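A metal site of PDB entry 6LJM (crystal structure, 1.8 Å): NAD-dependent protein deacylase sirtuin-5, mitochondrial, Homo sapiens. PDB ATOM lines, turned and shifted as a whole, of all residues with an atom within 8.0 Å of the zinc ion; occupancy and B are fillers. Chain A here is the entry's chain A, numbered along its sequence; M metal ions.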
ATOM      1  N   ARG A 135      20.561   2.956 -16.297  1.00  0.00           N
ATOM      2  CA  ARG A 135      21.804   3.468 -15.722  1.00  0.00           C
ATOM      3  C   ARG A 135      22.238   2.556 -14.593  1.00  0.00           C
ATOM      4  O   ARG A 135      21.427   2.187 -13.733  1.00  0.00           O
ATOM      5  CB  ARG A 135      21.658   4.894 -15.227  1.00  0.00           C
ATOM      6  CG  ARG A 135      22.992   5.414 -14.681  1.00  0.00           C
ATOM      7  CD  ARG A 135      23.049   6.868 -14.629  1.00  0.00           C
ATOM      8  NE  ARG A 135      22.447   7.419 -13.416  1.00  0.00           N
ATOM      9  CZ  ARG A 135      21.280   8.061 -13.362  1.00  0.00           C
ATOM     10  NH1 ARG A 135      20.543   8.195 -14.438  1.00  0.00           N
ATOM     11  NH2 ARG A 135      20.852   8.566 -12.217  1.00  0.00           N
ATOM     12  N   CYS A 136      23.510   2.167 -14.602  1.00  0.00           N
ATOM     13  CA  CYS A 136      24.019   1.295 -13.557  1.00  0.00           C
ATOM     14  C   CYS A 136      24.294   2.086 -12.287  1.00  0.00           C
ATOM     15  O   CYS A 136      25.045   3.074 -12.302  1.00  0.00           O
ATOM     16  CB  CYS A 136      25.293   0.565 -14.004  1.00  0.00           C
ATOM     17  SG  CYS A 136      25.870  -0.529 -12.797  1.00  0.00           S
ATOM     18  N   THR A 137      23.722   1.642 -11.172  1.00  0.00           N
ATOM     19  CA  THR A 137      23.919   2.361  -9.932  1.00  0.00           C
ATOM     20  C   THR A 137      25.312   2.135  -9.349  1.00  0.00           C
ATOM     21  O   THR A 137      25.667   2.764  -8.345  1.00  0.00           O
ATOM     22  CB  THR A 137      22.878   1.951  -8.898  1.00  0.00           C
ATOM     23  OG1 THR A 137      23.026   0.568  -8.591  1.00  0.00           O
ATOM     24  CG2 THR A 137      21.470   2.225  -9.420  1.00  0.00           C
ATOM     25  N   SER A 138      26.100   1.232  -9.928  1.00  0.00           N
ATOM     26  CA  SER A 138      27.484   1.029  -9.494  1.00  0.00           C
ATOM     27  C   SER A 138      28.479   1.727 -10.399  1.00  0.00           C
ATOM     28  O   SER A 138      29.296   2.518  -9.927  1.00  0.00           O
ATOM     29  CB  SER A 138      27.802  -0.464  -9.423  1.00  0.00           C
ATOM     30  OG  SER A 138      27.152  -1.073  -8.334  1.00  0.00           O
ATOM     31  N   CYS A 139      28.423   1.468 -11.710  1.00  0.00           N
ATOM     32  CA  CYS A 139      29.437   1.999 -12.605  1.00  0.00           C
ATOM     33  C   CYS A 139      28.982   3.207 -13.404  1.00  0.00           C
ATOM     34  O   CYS A 139      29.805   3.820 -14.071  1.00  0.00           O
ATOM     35  CB  CYS A 139      29.918   0.899 -13.567  1.00  0.00           C
ATOM     36  SG  CYS A 139      28.798   0.440 -14.942  1.00  0.00           S
ATOM     37  N   GLY A 140      27.694   3.581 -13.359  1.00  0.00           N
ATOM     38  CA  GLY A 140      27.210   4.754 -14.040  1.00  0.00           C
ATOM     39  C   GLY A 140      26.933   4.589 -15.515  1.00  0.00           C
ATOM     40  O   GLY A 140      26.454   5.551 -16.151  1.00  0.00           O
ATOM     41  N   VAL A 141      27.218   3.430 -16.108  1.00  0.00           N
ATOM     42  CA  VAL A 141      27.051   3.319 -17.564  1.00  0.00           C
ATOM     43  C   VAL A 141      25.580   3.454 -17.910  1.00  0.00           C
ATOM     44  O   VAL A 141      24.708   2.911 -17.220  1.00  0.00           O
ATOM     45  CB  VAL A 141      27.633   2.003 -18.092  1.00  0.00           C
ATOM     46  CG1 VAL A 141      27.287   1.786 -19.546  1.00  0.00           C
ATOM     47  CG2 VAL A 141      29.144   2.019 -17.938  1.00  0.00           C
ATOM     48  N   VAL A 142      25.296   4.206 -18.971  1.00  0.00           N
ATOM     49  CA  VAL A 142      23.944   4.367 -19.522  1.00  0.00           C
ATOM     50  C   VAL A 142      23.853   3.519 -20.780  1.00  0.00           C
ATOM     51  O   VAL A 142      24.726   3.582 -21.656  1.00  0.00           O
ATOM     52  CB  VAL A 142      23.638   5.849 -19.819  1.00  0.00           C
ATOM     53  CG1 VAL A 142      22.248   6.036 -20.454  1.00  0.00           C
ATOM     54  CG2 VAL A 142      23.789   6.691 -18.580  1.00  0.00           C
ATOM     55  N   ARG A 176      20.295  -6.240 -14.034  1.00  0.00           N
ATOM     56  CA  ARG A 176      21.683  -6.081 -13.622  1.00  0.00           C
ATOM     57  C   ARG A 176      22.530  -5.592 -14.788  1.00  0.00           C
ATOM     58  O   ARG A 176      22.220  -5.870 -15.950  1.00  0.00           O
ATOM     59  CB  ARG A 176      22.260  -7.395 -13.073  1.00  0.00           C
ATOM     60  CG  ARG A 176      21.427  -8.072 -11.962  1.00  0.00           C
ATOM     61  CD  ARG A 176      21.154  -7.169 -10.758  1.00  0.00           C
ATOM     62  NE  ARG A 176      22.384  -6.791 -10.046  1.00  0.00           N
ATOM     63  CZ  ARG A 176      22.453  -6.534  -8.738  1.00  0.00           C
ATOM     64  NH1 ARG A 176      21.357  -6.624  -7.981  1.00  0.00           N
ATOM     65  NH2 ARG A 176      23.627  -6.213  -8.196  1.00  0.00           N
ATOM     66  N   CYS A 177      23.610  -4.883 -14.457  1.00  0.00           N
ATOM     67  CA  CYS A 177      24.520  -4.333 -15.461  1.00  0.00           C
ATOM     68  C   CYS A 177      25.259  -5.450 -16.189  1.00  0.00           C
ATOM     69  O   CYS A 177      25.709  -6.413 -15.584  1.00  0.00           O
ATOM     70  CB  CYS A 177      25.516  -3.386 -14.776  1.00  0.00           C
ATOM     71  SG  CYS A 177      26.677  -2.593 -15.857  1.00  0.00           S
ATOM     72  N   GLU A 178      25.373  -5.332 -17.515  1.00  0.00           N
ATOM     73  CA  GLU A 178      25.997  -6.365 -18.323  1.00  0.00           C
ATOM     74  C   GLU A 178      27.375  -5.940 -18.808  1.00  0.00           C
ATOM     75  O   GLU A 178      27.967  -6.616 -19.661  1.00  0.00           O
ATOM     76  CB  GLU A 178      25.105  -6.738 -19.509  1.00  0.00           C
ATOM     77  CG  GLU A 178      23.832  -7.485 -19.100  1.00  0.00           C
ATOM     78  CD  GLU A 178      22.948  -7.817 -20.285  1.00  0.00           C
ATOM     79  OE1 GLU A 178      23.286  -8.766 -21.019  1.00  0.00           O
ATOM     80  OE2 GLU A 178      21.931  -7.117 -20.508  1.00  0.00           O
ATOM     81  N   GLU A 179      27.908  -4.829 -18.304  1.00  0.00           N
ATOM     82  CA  GLU A 179      29.317  -4.524 -18.538  1.00  0.00           C
ATOM     83  C   GLU A 179      30.181  -5.621 -17.923  1.00  0.00           C
ATOM     84  O   GLU A 179      29.900  -6.111 -16.822  1.00  0.00           O
ATOM     85  CB  GLU A 179      29.683  -3.170 -17.944  1.00  0.00           C
ATOM     86  CG  GLU A 179      28.916  -2.000 -18.509  1.00  0.00           C
ATOM     87  CD  GLU A 179      29.294  -1.740 -19.947  1.00  0.00           C
ATOM     88  OE1 GLU A 179      30.461  -1.375 -20.187  1.00  0.00           O
ATOM     89  OE2 GLU A 179      28.430  -1.923 -20.835  1.00  0.00           O
ATOM     90  N   ALA A 180      31.234  -6.000 -18.625  1.00  0.00           N
ATOM     91  CA  ALA A 180      32.184  -6.972 -18.110  1.00  0.00           C
ATOM     92  C   ALA A 180      32.708  -6.550 -16.738  1.00  0.00           C
ATOM     93  O   ALA A 180      33.279  -5.469 -16.583  1.00  0.00           O
ATOM     94  CB  ALA A 180      33.342  -7.124 -19.092  1.00  0.00           C
ATOM     95  N   GLY A 181      32.533  -7.417 -15.760  1.00  0.00           N
ATOM     96  CA  GLY A 181      33.024  -7.123 -14.438  1.00  0.00           C
ATOM     97  C   GLY A 181      32.254  -6.103 -13.646  1.00  0.00           C
ATOM     98  O   GLY A 181      32.815  -5.528 -12.731  1.00  0.00           O
ATOM     99  N   CYS A 182      30.974  -5.845 -13.957  1.00  0.00           N
ATOM    100  CA  CYS A 182      30.184  -4.969 -13.089  1.00  0.00           C
ATOM    101  C   CYS A 182      29.080  -5.734 -12.381  1.00  0.00           C
ATOM    102  O   CYS A 182      29.183  -5.970 -11.171  1.00  0.00           O
ATOM    103  CB  CYS A 182      29.618  -3.761 -13.830  1.00  0.00           C
ATOM    104  SG  CYS A 182      28.856  -2.680 -12.606  1.00  0.00           S
ATOM    105  N   GLY A 183      27.999  -6.102 -13.060  1.00  0.00           N
ATOM    106  CA  GLY A 183      26.895  -6.762 -12.365  1.00  0.00           C
ATOM    107  C   GLY A 183      26.088  -5.924 -11.382  1.00  0.00           C
ATOM    108  O   GLY A 183      25.241  -6.489 -10.664  1.00  0.00           O
ATOM    109  N   GLY A 184      26.283  -4.607 -11.338  1.00  0.00           N
ATOM    110  CA  GLY A 184      25.535  -3.769 -10.420  1.00  0.00           C
ATOM    111  C   GLY A 184      24.055  -3.702 -10.755  1.00  0.00           C
ATOM    112  O   GLY A 184      23.605  -4.106 -11.825  1.00  0.00           O
ATOM    113  N   LEU A 185      23.294  -3.163  -9.801  1.00  0.00           N
ATOM    114  CA  LEU A 185      21.849  -3.021  -9.977  1.00  0.00           C
ATOM    115  C   LEU A 185      21.535  -1.837 -10.881  1.00  0.00           C
ATOM    116  O   LEU A 185      22.014  -0.707 -10.650  1.00  0.00           O
ATOM    117  CB  LEU A 185      21.173  -2.870  -8.603  1.00  0.00           C
ATOM    118  CG  LEU A 185      19.677  -2.531  -8.602  1.00  0.00           C
ATOM    119  CD1 LEU A 185      18.833  -3.707  -9.136  1.00  0.00           C
ATOM    120  CD2 LEU A 185      19.245  -2.162  -7.190  1.00  0.00           C
ATOM    121  N   LEU A 186      20.752  -2.075 -11.923  1.00  0.00           N
ATOM    122  CA  LEU A 186      20.339  -1.012 -12.815  1.00  0.00           C
ATOM    123  C   LEU A 186      19.121  -0.287 -12.253  1.00  0.00           C
ATOM    124  O   LEU A 186      18.299  -0.848 -11.522  1.00  0.00           O
ATOM    125  CB  LEU A 186      19.970  -1.529 -14.213  1.00  0.00           C
ATOM    126  CG  LEU A 186      21.060  -2.333 -14.922  1.00  0.00           C
ATOM    127  CD1 LEU A 186      20.511  -2.724 -16.300  1.00  0.00           C
ATOM    128  CD2 LEU A 186      22.338  -1.499 -15.026  1.00  0.00           C
HETATM  129 ZN    ZN M   1      27.651  -1.321 -14.084  1.00  0.00          ZN
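The side-chain sulfur (SG) of Cys 139 sits close to the backbone NH (N) of Val 141 (3.6 Å). The side-chain sulfur (SG) of Cys 136 sits close to the backbone NH (N) of Ser 138. O of Val 141 lies within hydrogen-bond range of N of Cys 136. The side-chain sulfur (SG) of Cys 182 sits close to the backbone NH (N) of Gly 184, 3.5 Å away. The backbone NH (N) of Cys 177 lies within hydrogen-bond range of the backbone carbonyl oxygen (O) of Gly 184, 2.7 Å away. N of Glu 179 lies close to SG of Cys 177. The backbone NH (N) of Gly 183 is in hydrogen-bond range of the backbone carbonyl oxygen (O) of Cys 177, 3.4 Å away.
Four residues have an atom within 4 Å of the zinc ion: Cys 136, Cys 139, Cys 177 and Cys 182.
The zinc ion is bound by SG of Cys 139 (2.3 Å), SG of Cys 136 (2.3 Å), SG of Cys 182 (2.3 Å) and SG of Cys 177 (2.4 Å).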
